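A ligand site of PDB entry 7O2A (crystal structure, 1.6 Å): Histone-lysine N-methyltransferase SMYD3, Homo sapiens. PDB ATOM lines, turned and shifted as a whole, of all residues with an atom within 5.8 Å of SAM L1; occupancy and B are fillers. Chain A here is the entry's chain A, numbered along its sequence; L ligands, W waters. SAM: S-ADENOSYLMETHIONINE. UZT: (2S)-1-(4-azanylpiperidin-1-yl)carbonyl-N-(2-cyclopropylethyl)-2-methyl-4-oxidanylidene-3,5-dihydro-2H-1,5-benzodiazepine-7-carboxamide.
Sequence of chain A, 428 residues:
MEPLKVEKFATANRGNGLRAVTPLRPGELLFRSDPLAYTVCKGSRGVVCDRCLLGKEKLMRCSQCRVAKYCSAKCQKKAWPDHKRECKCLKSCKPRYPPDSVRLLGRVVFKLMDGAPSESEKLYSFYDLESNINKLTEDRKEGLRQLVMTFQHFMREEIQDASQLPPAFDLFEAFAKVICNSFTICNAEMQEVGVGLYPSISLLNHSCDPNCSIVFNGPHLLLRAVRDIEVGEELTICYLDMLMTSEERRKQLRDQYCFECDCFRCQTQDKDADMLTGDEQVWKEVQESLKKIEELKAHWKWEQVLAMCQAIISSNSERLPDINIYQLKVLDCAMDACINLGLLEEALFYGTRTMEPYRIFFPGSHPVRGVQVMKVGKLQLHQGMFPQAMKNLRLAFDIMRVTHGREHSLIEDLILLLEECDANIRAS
An oxygen (O3') of SAM L1 sits at hydrogen-bond distance from the backbone carbonyl oxygen of Tyr 257.
An oxygen (OXT) of SAM L1 is in hydrogen-bond range of the side-chain hydroxyl of Tyr 124 (2.7 Å).
The backbone carbonyl oxygen of Arg 14 sits at hydrogen-bond distance from a nitrogen (N) of SAM L1, 2.7 Å away.
The backbone NH of Asn 16 lies within hydrogen-bond range of an oxygen (O) of SAM L1 (2.8 Å).
O of Asn 16 lies within hydrogen-bond range of N of SAM L1, at 2.8 Å.
The side-chain amide oxygen (OD1) of Asn 205 is in hydrogen-bond range of a nitrogen (N) of SAM L1 (2.8 Å).
An oxygen (O3') of SAM L1 is in hydrogen-bond range of the side-chain amide nitrogen (ND2) of Asn 132 (2.9 Å).
N7 of SAM L1 lies within hydrogen-bond range of N of His 206, 3.0 Å away.
The backbone carbonyl oxygen (O) of His 206 sits at hydrogen-bond distance from a nitrogen (N6) of SAM L1 (3.0 Å).
N6 of UZT L2 sits at hydrogen-bond distance from O of Tyr 239.
The backbone carbonyl oxygen of Tyr 257 lies within hydrogen-bond range of the side-chain amide nitrogen of Asn 132, at 3.4 Å.
The side-chain hydroxyl of Tyr 124 lies within hydrogen-bond range of the side-chain amide oxygen of Asn 16 (3.0 Å).
The side-chain hydroxyl (OH) of Tyr 124 is in hydrogen-bond range of the backbone carbonyl oxygen (O) of Asp 128, 3.2 Å away.
The backbone carbonyl oxygen (O) of Arg 14 sits close to the side-chain amide oxygen (OD1) of Asn 205, 3.5 Å away.
N of Asn 132 sits at hydrogen-bond distance from OE2 of Glu 130.
SG of Cys 180 sits at hydrogen-bond distance from ND2 of Asn 181, 3.5 Å away.
The side-chain amide nitrogen (ND2) of Asn 181 sits at hydrogen-bond distance from the backbone carbonyl oxygen (O) of Glu 130, 3.0 Å away.
The backbone carbonyl oxygen of Leu 204 sits at hydrogen-bond distance from the side-chain hydroxyl of Tyr 239 (2.6 Å).
The side-chain amide oxygen (OD1) of Asn 181 lies close to a sulfur (SD) of SAM L1 (3.6 Å).
O of Ser 202 sits close to SD of SAM L1, at 3.4 Å.
OH of Tyr 239 sits close to SD of SAM L1 (3.6 Å).
Gly 15 touches SAM L1.
Glu 130 touches SAM L1.
Cys 180 touches SAM L1 (O to CE, 3.5 Å).
Leu 203 touches SAM L1 (O to CB, 3.6 Å).
Leu 204 touches SAM L1.
Phe 259 touches SAM L1.
Of the 26 residues printed, 16 come within 4 Å of SAM L1.
Along chain A the residues within 4 Å of SAM L1 span positions 14 to 259.
The nearest printed residue that does not touch SAM L1 is Asn 13 (4.3 Å).
Water W7 lies within hydrogen-bond range of an oxygen (O) of SAM L1 (2.6 Å) and the side-chain carboxylate (OE1) of Glu 130 (3.0 Å).
Water W4 lies within hydrogen-bond range of O of Cys 258 (2.7 Å), O2' of SAM L1 (2.8 Å), NZ of Lys 135 (2.8 Å) and OD1 of Asn 132 (3.2 Å).
Water W1 lies within hydrogen-bond range of the side-chain amide oxygen (OD1) of Asn 181 (2.8 Å), an oxygen (OXT) of SAM L1 (2.8 Å) and the backbone NH (N) of Glu 130 (2.8 Å).
Water W5 bridges a nitrogen (N1) of SAM L1 (2.8 Å) and the backbone carbonyl oxygen (O) of Glu 260 (3.1 Å).
Water W2 lies within hydrogen-bond range of OE1 of Glu 130 (2.9 Å), N of SAM L1 (2.9 Å) and O of Arg 14 (3.4 Å).
Water W3 lies within hydrogen-bond range of a nitrogen (N6) of SAM L1 and the guanidinium group (NH1) of Arg 14.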
ATOM      1  N   ASN A  13     -21.728 -15.820   8.823  1.00  0.00           N
ATOM      2  CA  ASN A  13     -20.812 -16.655   9.589  1.00  0.00           C
ATOM      3  C   ASN A  13     -21.384 -17.888  10.268  1.00  0.00           C
ATOM      4  O   ASN A  13     -20.753 -18.481  11.197  1.00  0.00           O
ATOM      5  CB  ASN A  13     -20.064 -15.805  10.623  1.00  0.00           C
ATOM      6  CG  ASN A  13     -20.957 -15.228  11.727  1.00  0.00           C
ATOM      7  OD1 ASN A  13     -22.094 -15.630  11.903  1.00  0.00           O
ATOM      8  ND2 ASN A  13     -20.504 -14.154  12.356  1.00  0.00           N
ATOM      9  N   ARG A  14     -22.548 -18.311   9.778  1.00  0.00           N
ATOM     10  CA  ARG A  14     -23.105 -19.541  10.293  1.00  0.00           C
ATOM     11  C   ARG A  14     -23.705 -20.420   9.235  1.00  0.00           C
ATOM     12  O   ARG A  14     -24.693 -21.177   9.460  1.00  0.00           O
ATOM     13  CB  ARG A  14     -23.949 -19.307  11.472  1.00  0.00           C
ATOM     14  CG  ARG A  14     -25.040 -18.320  11.307  1.00  0.00           C
ATOM     15  CD  ARG A  14     -24.898 -17.417  12.487  1.00  0.00           C
ATOM     16  NE  ARG A  14     -26.188 -17.058  12.908  1.00  0.00           N
ATOM     17  CZ  ARG A  14     -26.501 -16.597  14.102  1.00  0.00           C
ATOM     18  NH1 ARG A  14     -25.596 -16.416  15.040  1.00  0.00           N
ATOM     19  NH2 ARG A  14     -27.776 -16.305  14.324  1.00  0.00           N
ATOM     20  N   GLY A  15     -23.073 -20.433   8.096  1.00  0.00           N
ATOM     21  CA  GLY A  15     -23.509 -21.282   7.023  1.00  0.00           C
ATOM     22  C   GLY A  15     -24.792 -20.822   6.424  1.00  0.00           C
ATOM     23  O   GLY A  15     -24.994 -19.609   6.303  1.00  0.00           O
ATOM     24  N   ASN A  16     -25.583 -21.769   5.926  1.00  0.00           N
ATOM     25  CA  ASN A  16     -26.910 -21.458   5.412  1.00  0.00           C
ATOM     26  C   ASN A  16     -27.863 -21.251   6.562  1.00  0.00           C
ATOM     27  O   ASN A  16     -27.626 -21.771   7.663  1.00  0.00           O
ATOM     28  CB  ASN A  16     -27.446 -22.531   4.469  1.00  0.00           C
ATOM     29  CG  ASN A  16     -26.547 -22.695   3.281  1.00  0.00           C
ATOM     30  OD1 ASN A  16     -26.119 -23.811   2.998  1.00  0.00           O
ATOM     31  ND2 ASN A  16     -26.126 -21.605   2.704  1.00  0.00           N
ATOM     32  N   GLY A  17     -28.921 -20.489   6.303  1.00  0.00           N
ATOM     33  CA  GLY A  17     -29.947 -20.172   7.292  1.00  0.00           C
ATOM     34  C   GLY A  17     -31.278 -19.965   6.650  1.00  0.00           C
ATOM     35  O   GLY A  17     -31.401 -20.111   5.442  1.00  0.00           O
ATOM     36  N   TYR A 124     -34.241 -27.706   1.270  1.00  0.00           N
ATOM     37  CA  TYR A 124     -32.878 -28.145   1.540  1.00  0.00           C
ATOM     38  C   TYR A 124     -32.982 -29.659   1.717  1.00  0.00           C
ATOM     39  O   TYR A 124     -33.931 -30.174   2.325  1.00  0.00           O
ATOM     40  CB  TYR A 124     -32.461 -27.504   2.881  1.00  0.00           C
ATOM     41  CG  TYR A 124     -30.959 -27.319   3.214  1.00  0.00           C
ATOM     42  CD1 TYR A 124     -30.087 -26.608   2.378  1.00  0.00           C
ATOM     43  CD2 TYR A 124     -30.503 -27.650   4.453  1.00  0.00           C
ATOM     44  CE1 TYR A 124     -28.805 -26.313   2.733  1.00  0.00           C
ATOM     45  CE2 TYR A 124     -29.209 -27.372   4.831  1.00  0.00           C
ATOM     46  CZ  TYR A 124     -28.366 -26.684   3.993  1.00  0.00           C
ATOM     47  OH  TYR A 124     -27.095 -26.315   4.366  1.00  0.00           O
ATOM     48  N   ASP A 128     -27.605 -31.761   1.048  1.00  0.00           N
ATOM     49  CA  ASP A 128     -27.152 -30.418   1.380  1.00  0.00           C
ATOM     50  C   ASP A 128     -26.755 -30.198   2.824  1.00  0.00           C
ATOM     51  O   ASP A 128     -26.157 -29.154   3.129  1.00  0.00           O
ATOM     52  CB  ASP A 128     -28.293 -29.400   1.110  1.00  0.00           C
ATOM     53  CG  ASP A 128     -28.772 -29.402  -0.370  1.00  0.00           C
ATOM     54  OD1 ASP A 128     -27.925 -29.466  -1.314  1.00  0.00           O
ATOM     55  OD2 ASP A 128     -29.998 -29.250  -0.538  1.00  0.00           O
ATOM     56  N   LEU A 129     -27.154 -31.086   3.733  1.00  0.00           N
ATOM     57  CA  LEU A 129     -27.004 -30.794   5.165  1.00  0.00           C
ATOM     58  C   LEU A 129     -25.528 -30.584   5.582  1.00  0.00           C
ATOM     59  O   LEU A 129     -24.593 -31.229   5.082  1.00  0.00           O
ATOM     60  CB  LEU A 129     -27.535 -31.902   6.042  1.00  0.00           C
ATOM     61  CG  LEU A 129     -29.003 -32.215   5.925  1.00  0.00           C
ATOM     62  CD1 LEU A 129     -29.400 -33.434   6.796  1.00  0.00           C
ATOM     63  CD2 LEU A 129     -29.848 -31.039   6.365  1.00  0.00           C
ATOM     64  N   GLU A 130     -25.373 -29.761   6.583  1.00  0.00           N
ATOM     65  CA  GLU A 130     -24.066 -29.480   7.183  1.00  0.00           C
ATOM     66  C   GLU A 130     -23.579 -30.727   7.921  1.00  0.00           C
ATOM     67  O   GLU A 130     -24.325 -31.377   8.618  1.00  0.00           O
ATOM     68  CB  GLU A 130     -24.233 -28.352   8.161  1.00  0.00           C
ATOM     69  CG  GLU A 130     -22.956 -28.023   8.964  1.00  0.00           C
ATOM     70  CD  GLU A 130     -21.889 -27.483   8.066  1.00  0.00           C
ATOM     71  OE1 GLU A 130     -22.070 -26.308   7.691  1.00  0.00           O
ATOM     72  OE2 GLU A 130     -20.909 -28.180   7.740  1.00  0.00           O
ATOM     73  N   ASN A 132     -20.110 -30.440   9.251  1.00  0.00           N
ATOM     74  CA  ASN A 132     -18.973 -29.956  10.055  1.00  0.00           C
ATOM     75  C   ASN A 132     -17.781 -30.864  10.078  1.00  0.00           C
ATOM     76  O   ASN A 132     -17.053 -30.889  11.040  1.00  0.00           O
ATOM     77  CB  ASN A 132     -19.402 -29.687  11.532  1.00  0.00           C
ATOM     78  CG  ASN A 132     -20.337 -28.516  11.649  1.00  0.00           C
ATOM     79  OD1 ASN A 132     -20.094 -27.486  11.037  1.00  0.00           O
ATOM     80  ND2 ASN A 132     -21.441 -28.701  12.301  1.00  0.00           N
ATOM     81  N   LYS A 135     -14.431 -29.564  11.341  1.00  0.00           N
ATOM     82  CA  LYS A 135     -14.332 -29.216  12.774  1.00  0.00           C
ATOM     83  C   LYS A 135     -14.360 -30.423  13.709  1.00  0.00           C
ATOM     84  O   LYS A 135     -14.153 -30.260  14.932  1.00  0.00           O
ATOM     85  CB  LYS A 135     -15.407 -28.242  13.175  1.00  0.00           C
ATOM     86  CG  LYS A 135     -15.268 -26.910  12.506  1.00  0.00           C
ATOM     87  CD  LYS A 135     -16.500 -26.078  12.759  1.00  0.00           C
ATOM     88  CE  LYS A 135     -16.309 -24.715  12.070  1.00  0.00           C
ATOM     89  NZ  LYS A 135     -17.388 -23.877  12.669  1.00  0.00           N
ATOM     90  N   CYS A 180     -25.585 -33.429  13.828  1.00  0.00           N
ATOM     91  CA  CYS A 180     -25.898 -32.037  14.026  1.00  0.00           C
ATOM     92  C   CYS A 180     -27.211 -31.591  13.367  1.00  0.00           C
ATOM     93  O   CYS A 180     -27.502 -30.401  13.412  1.00  0.00           O
ATOM     94  CB  CYS A 180     -24.761 -31.146  13.624  1.00  0.00           C
ATOM     95  SG  CYS A 180     -24.373 -31.228  11.847  1.00  0.00           S
ATOM     96  N   ASN A 181     -27.970 -32.522  12.784  1.00  0.00           N
ATOM     97  CA  ASN A 181     -29.292 -32.205  12.220  1.00  0.00           C
ATOM     98  C   ASN A 181     -30.442 -33.067  12.724  1.00  0.00           C
ATOM     99  O   ASN A 181     -31.549 -32.902  12.273  1.00  0.00           O
ATOM    100  CB  ASN A 181     -29.236 -32.323  10.723  1.00  0.00           C
ATOM    101  CG  ASN A 181     -28.336 -31.316  10.090  1.00  0.00           C
ATOM    102  OD1 ASN A 181     -28.712 -30.188   9.947  1.00  0.00           O
ATOM    103  ND2 ASN A 181     -27.125 -31.706   9.741  1.00  0.00           N
ATOM    104  N   SER A 202     -33.941 -28.013   8.948  1.00  0.00           N
ATOM    105  CA  SER A 202     -32.581 -28.058   9.385  1.00  0.00           C
ATOM    106  C   SER A 202     -31.798 -26.821   8.956  1.00  0.00           C
ATOM    107  O   SER A 202     -30.688 -26.588   9.416  1.00  0.00           O
ATOM    108  CB  SER A 202     -31.843 -29.230   8.780  1.00  0.00           C
ATOM    109  OG  SER A 202     -32.218 -30.460   9.296  1.00  0.00           O
ATOM    110  N   LEU A 203     -32.363 -25.996   8.102  1.00  0.00           N
ATOM    111  CA  LEU A 203     -31.805 -24.659   7.838  1.00  0.00           C
ATOM    112  C   LEU A 203     -31.744 -23.714   9.032  1.00  0.00           C
ATOM    113  O   LEU A 203     -30.902 -22.793   9.020  1.00  0.00           O
ATOM    114  CB  LEU A 203     -32.489 -23.970   6.671  1.00  0.00           C
ATOM    115  CG  LEU A 203     -32.059 -24.455   5.291  1.00  0.00           C
ATOM    116  CD1 LEU A 203     -33.094 -23.946   4.283  1.00  0.00           C
ATOM    117  CD2 LEU A 203     -30.628 -24.099   4.950  1.00  0.00           C
ATOM    118  N   LEU A 204     -32.609 -23.937  10.024  1.00  0.00           N
ATOM    119  CA  LEU A 204     -32.635 -23.047  11.191  1.00  0.00           C
ATOM    120  C   LEU A 204     -31.363 -23.103  11.978  1.00  0.00           C
ATOM    121  O   LEU A 204     -30.979 -24.185  12.530  1.00  0.00           O
ATOM    122  CB  LEU A 204     -33.772 -23.383  12.186  1.00  0.00           C
ATOM    123  CG  LEU A 204     -35.182 -23.228  11.549  1.00  0.00           C
ATOM    124  CD1 LEU A 204     -36.223 -24.017  12.314  1.00  0.00           C
ATOM    125  CD2 LEU A 204     -35.523 -21.736  11.566  1.00  0.00           C
ATOM    126  N   ASN A 205     -30.761 -21.933  12.142  1.00  0.00           N
ATOM    127  CA  ASN A 205     -29.708 -21.767  13.108  1.00  0.00           C
ATOM    128  C   ASN A 205     -30.195 -21.604  14.560  1.00  0.00           C
ATOM    129  O   ASN A 205     -31.339 -21.328  14.783  1.00  0.00           O
ATOM    130  CB  ASN A 205     -28.711 -20.681  12.660  1.00  0.00           C
ATOM    131  CG  ASN A 205     -27.931 -21.123  11.438  1.00  0.00           C
ATOM    132  OD1 ASN A 205     -27.364 -22.224  11.404  1.00  0.00           O
ATOM    133  ND2 ASN A 205     -27.904 -20.290  10.417  1.00  0.00           N
ATOM    134  N   HIS A 206     -29.257 -21.765  15.474  1.00  0.00           N
ATOM    135  CA  HIS A 206     -29.486 -21.717  16.929  1.00  0.00           C
ATOM    136  C   HIS A 206     -29.417 -20.294  17.503  1.00  0.00           C
ATOM    137  O   HIS A 206     -28.535 -19.529  17.150  1.00  0.00           O
ATOM    138  CB  HIS A 206     -28.425 -22.542  17.636  1.00  0.00           C
ATOM    139  CG  HIS A 206     -28.409 -22.330  19.145  1.00  0.00           C
ATOM    140  ND1 HIS A 206     -29.296 -22.951  19.971  1.00  0.00           N
ATOM    141  CD2 HIS A 206     -27.683 -21.506  19.930  1.00  0.00           C
ATOM    142  CE1 HIS A 206     -29.116 -22.561  21.201  1.00  0.00           C
ATOM    143  NE2 HIS A 206     -28.119 -21.707  21.207  1.00  0.00           N
ATOM    144  N   SER A 207     -30.277 -19.990  18.473  1.00  0.00           N
ATOM    145  CA  SER A 207     -30.105 -18.871  19.380  1.00  0.00           C
ATOM    146  C   SER A 207     -30.467 -19.303  20.779  1.00  0.00           C
ATOM    147  O   SER A 207     -31.416 -20.069  20.991  1.00  0.00           O
ATOM    148  CB  SER A 207     -31.015 -17.705  18.962  1.00  0.00           C
ATOM    149  OG  SER A 207     -31.010 -16.695  19.920  1.00  0.00           O
ATOM    150  N   TYR A 239     -31.728 -24.788  20.029  1.00  0.00           N
ATOM    151  CA  TYR A 239     -31.499 -26.213  19.858  1.00  0.00           C
ATOM    152  C   TYR A 239     -31.602 -27.009  21.178  1.00  0.00           C
ATOM    153  O   TYR A 239     -31.696 -28.273  21.154  1.00  0.00           O
ATOM    154  CB  TYR A 239     -30.125 -26.516  19.273  1.00  0.00           C
ATOM    155  CG  TYR A 239     -29.871 -26.060  17.849  1.00  0.00           C
ATOM    156  CD1 TYR A 239     -30.824 -25.465  17.074  1.00  0.00           C
ATOM    157  CD2 TYR A 239     -28.618 -26.279  17.278  1.00  0.00           C
ATOM    158  CE1 TYR A 239     -30.558 -25.093  15.748  1.00  0.00           C
ATOM    159  CE2 TYR A 239     -28.327 -25.898  15.988  1.00  0.00           C
ATOM    160  CZ  TYR A 239     -29.300 -25.293  15.253  1.00  0.00           C
ATOM    161  OH  TYR A 239     -28.974 -24.974  13.959  1.00  0.00           O
ATOM    162  N   GLN A 256     -21.633 -31.310  19.920  1.00  0.00           N
ATOM    163  CA  GLN A 256     -22.628 -31.775  19.014  1.00  0.00           C
ATOM    164  C   GLN A 256     -22.674 -30.935  17.749  1.00  0.00           C
ATOM    165  O   GLN A 256     -22.809 -31.497  16.654  1.00  0.00           O
ATOM    166  CB  GLN A 256     -23.981 -31.850  19.680  1.00  0.00           C
ATOM    167  CG  GLN A 256     -25.014 -32.531  18.810  1.00  0.00           C
ATOM    168  CD  GLN A 256     -26.333 -32.779  19.519  1.00  0.00           C
ATOM    169  OE1 GLN A 256     -26.470 -32.530  20.745  1.00  0.00           O
ATOM    170  NE2 GLN A 256     -27.287 -33.284  18.781  1.00  0.00           N
ATOM    171  N   TYR A 257     -22.516 -29.612  17.875  1.00  0.00           N
ATOM    172  CA  TYR A 257     -22.790 -28.674  16.789  1.00  0.00           C
ATOM    173  C   TYR A 257     -21.581 -27.964  16.212  1.00  0.00           C
ATOM    174  O   TYR A 257     -21.710 -27.198  15.286  1.00  0.00           O
ATOM    175  CB  TYR A 257     -23.920 -27.693  17.176  1.00  0.00           C
ATOM    176  CG  TYR A 257     -25.243 -28.408  17.468  1.00  0.00           C
ATOM    177  CD1 TYR A 257     -26.054 -28.871  16.418  1.00  0.00           C
ATOM    178  CD2 TYR A 257     -25.672 -28.624  18.760  1.00  0.00           C
ATOM    179  CE1 TYR A 257     -27.175 -29.539  16.654  1.00  0.00           C
ATOM    180  CE2 TYR A 257     -26.860 -29.286  19.003  1.00  0.00           C
ATOM    181  CZ  TYR A 257     -27.600 -29.724  17.943  1.00  0.00           C
ATOM    182  OH  TYR A 257     -28.813 -30.454  18.129  1.00  0.00           O
ATOM    183  N   CYS A 258     -20.446 -28.070  16.895  1.00  0.00           N
ATOM    184  CA  CYS A 258     -19.198 -27.494  16.433  1.00  0.00           C
ATOM    185  C   CYS A 258     -19.271 -25.992  16.247  1.00  0.00           C
ATOM    186  O   CYS A 258     -18.836 -25.487  15.239  1.00  0.00           O
ATOM    187  CB  CYS A 258     -18.682 -28.178  15.093  1.00  0.00           C
ATOM    188  SG  CYS A 258     -18.203 -29.902  15.353  1.00  0.00           S
ATOM    189  N   PHE A 259     -19.907 -25.249  17.182  1.00  0.00           N
ATOM    190  CA  PHE A 259     -19.748 -23.826  17.207  1.00  0.00           C
ATOM    191  C   PHE A 259     -19.716 -23.268  18.628  1.00  0.00           C
ATOM    192  O   PHE A 259     -20.069 -23.981  19.615  1.00  0.00           O
ATOM    193  CB  PHE A 259     -20.818 -23.089  16.343  1.00  0.00           C
ATOM    194  CG  PHE A 259     -22.205 -23.066  16.929  1.00  0.00           C
ATOM    195  CD1 PHE A 259     -22.630 -21.962  17.664  1.00  0.00           C
ATOM    196  CD2 PHE A 259     -23.053 -24.140  16.786  1.00  0.00           C
ATOM    197  CE1 PHE A 259     -23.927 -21.969  18.211  1.00  0.00           C
ATOM    198  CE2 PHE A 259     -24.341 -24.152  17.349  1.00  0.00           C
ATOM    199  CZ  PHE A 259     -24.788 -23.059  17.998  1.00  0.00           C
ATOM    200  N   GLU A 260     -19.199 -22.042  18.666  1.00  0.00           N
ATOM    201  CA  GLU A 260     -19.055 -21.203  19.848  1.00  0.00           C
ATOM    202  C   GLU A 260     -20.116 -20.099  19.752  1.00  0.00           C
ATOM    203  O   GLU A 260     -20.264 -19.464  18.757  1.00  0.00           O
ATOM    204  CB  GLU A 260     -17.674 -20.526  19.824  1.00  0.00           C
ATOM    205  CG  GLU A 260     -16.514 -21.463  19.433  1.00  0.00           C
ATOM    206  CD  GLU A 260     -16.261 -22.614  20.377  1.00  0.00           C
ATOM    207  OE1 GLU A 260     -16.817 -22.613  21.527  1.00  0.00           O
ATOM    208  OE2 GLU A 260     -15.493 -23.540  19.956  1.00  0.00           O
ATOM    209  N   CYS A 261     -20.834 -19.873  20.831  1.00  0.00           N
ATOM    210  CA  CYS A 261     -21.831 -18.792  20.895  1.00  0.00           C
ATOM    211  C   CYS A 261     -21.333 -17.583  21.651  1.00  0.00           C
ATOM    212  O   CYS A 261     -20.869 -17.722  22.792  1.00  0.00           O
ATOM    213  CB  CYS A 261     -23.091 -19.339  21.591  1.00  0.00           C
ATOM    214  SG  CYS A 261     -24.447 -18.093  21.390  1.00  0.00           S
HETATM  215  N   SAM L   1     -26.051 -23.499   9.278  1.00  0.00           N
HETATM  216  CA  SAM L   1     -26.589 -24.810   8.898  1.00  0.00           C
HETATM  217  C   SAM L   1     -26.339 -25.148   7.444  1.00  0.00           C
HETATM  218  O   SAM L   1     -25.560 -24.431   6.797  1.00  0.00           O
HETATM  219  OXT SAM L   1     -26.874 -26.178   7.010  1.00  0.00           O
HETATM  220  CB  SAM L   1     -28.063 -24.918   9.274  1.00  0.00           C
HETATM  221  CG  SAM L   1     -28.289 -25.356  10.736  1.00  0.00           C
HETATM  222  SD  SAM L   1     -27.761 -26.961  11.150  1.00  0.00           S
HETATM  223  CE  SAM L   1     -29.075 -27.721  11.893  1.00  0.00           C
HETATM  224  C5' SAM L   1     -26.622 -26.856  12.468  1.00  0.00           C
HETATM  225  C4' SAM L   1     -25.278 -26.215  12.212  1.00  0.00           C
HETATM  226  O4' SAM L   1     -25.426 -24.845  11.870  1.00  0.00           O
HETATM  227  C3' SAM L   1     -24.319 -26.178  13.420  1.00  0.00           C
HETATM  228  O3' SAM L   1     -23.728 -27.467  13.660  1.00  0.00           O
HETATM  229  C2' SAM L   1     -23.335 -25.128  13.016  1.00  0.00           C
HETATM  230  O2' SAM L   1     -22.510 -25.529  11.926  1.00  0.00           O
HETATM  231  C1' SAM L   1     -24.351 -24.100  12.471  1.00  0.00           C
HETATM  232  N9  SAM L   1     -24.936 -23.212  13.520  1.00  0.00           N
HETATM  233  C8  SAM L   1     -26.198 -23.228  13.994  1.00  0.00           C
HETATM  234  N7  SAM L   1     -26.411 -22.208  14.818  1.00  0.00           N
HETATM  235  C5  SAM L   1     -25.293 -21.461  14.815  1.00  0.00           C
HETATM  236  C6  SAM L   1     -24.855 -20.285  15.487  1.00  0.00           C
HETATM  237  N6  SAM L   1     -25.660 -19.603  16.309  1.00  0.00           N
HETATM  238  N1  SAM L   1     -23.610 -19.889  15.293  1.00  0.00           N
HETATM  239  C2  SAM L   1     -22.769 -20.508  14.472  1.00  0.00           C
HETATM  240  N3  SAM L   1     -23.074 -21.617  13.803  1.00  0.00           N
HETATM  241  C4  SAM L   1     -24.305 -22.107  13.970  1.00  0.00           C
HETATM  242  C4  UZT L   2     -32.551 -29.046  16.479  1.00  0.00           C
HETATM  243  C5  UZT L   2     -32.100 -29.788  17.730  1.00  0.00           C
HETATM  244  C7  UZT L   2     -34.217 -30.322  18.865  1.00  0.00           C
HETATM  245  C10 UZT L   2     -34.877 -29.254  21.067  1.00  0.00           C
HETATM  246  C13 UZT L   2     -37.360 -30.599  20.967  1.00  0.00           C
HETATM  247  C17 UZT L   2     -39.848 -29.267  21.488  1.00  0.00           C
HETATM  248  C20 UZT L   2     -38.991 -27.448  22.910  1.00  0.00           C
HETATM  249  C21 UZT L   2     -37.453 -29.768  24.351  1.00  0.00           C
HETATM  250  C24 UZT L   2     -35.589 -31.302  23.758  1.00  0.00           C
HETATM  251  C26 UZT L   2     -35.290 -32.852  25.847  1.00  0.00           C
HETATM  252  C28 UZT L   2     -35.903 -30.493  26.045  1.00  0.00           C
HETATM  253  C1  UZT L   2     -31.707 -28.589  14.090  1.00  0.00           C
HETATM  254  C2  UZT L   2     -30.456 -29.053  14.901  1.00  0.00           C
HETATM  255  C3  UZT L   2     -31.839 -29.596  15.201  1.00  0.00           C
HETATM  256  N6  UZT L   2     -33.048 -29.687  18.879  1.00  0.00           N
HETATM  257  O8  UZT L   2     -34.501 -31.117  17.973  1.00  0.00           O
HETATM  258  C9  UZT L   2     -35.178 -30.096  19.978  1.00  0.00           C
HETATM  259  C14 UZT L   2     -36.408 -30.743  19.947  1.00  0.00           C
HETATM  260  C11 UZT L   2     -35.855 -29.102  22.082  1.00  0.00           C
HETATM  261  C12 UZT L   2     -37.102 -29.850  22.052  1.00  0.00           C
HETATM  262  N15 UZT L   2     -38.505 -31.295  20.895  1.00  0.00           N
HETATM  263  C16 UZT L   2     -39.706 -30.750  21.180  1.00  0.00           C
HETATM  264  O30 UZT L   2     -40.679 -31.487  21.126  1.00  0.00           O
HETATM  265  C18 UZT L   2     -39.207 -28.899  22.896  1.00  0.00           C
HETATM  266  N19 UZT L   2     -37.911 -29.606  23.117  1.00  0.00           N
HETATM  267  O22 UZT L   2     -38.077 -29.324  25.349  1.00  0.00           O
HETATM  268  N23 UZT L   2     -36.409 -30.557  24.669  1.00  0.00           N
HETATM  269  C25 UZT L   2     -35.909 -32.677  24.363  1.00  0.00           C
HETATM  270  N29 UZT L   2     -35.840 -34.035  26.566  1.00  0.00           N
HETATM  271  C27 UZT L   2     -35.643 -31.739  26.785  1.00  0.00           C
HETATM  272  O   HOH W   1     -27.708 -28.723   7.809  1.00  0.00           O
HETATM  273  O   HOH W   2     -23.223 -24.269   9.370  1.00  0.00           O
HETATM  274  O   HOH W   3     -24.949 -17.433  18.282  1.00  0.00           O
HETATM  275  O   HOH W   4     -19.985 -24.911  12.921  1.00  0.00           O
HETATM  276  O   HOH W   5     -21.983 -18.043  16.631  1.00  0.00           O
HETATM  277  O   HOH W   6     -20.685 -22.239  12.453  1.00  0.00           O
HETATM  278  O   HOH W   7     -23.657 -25.487   5.337  1.00  0.00           O
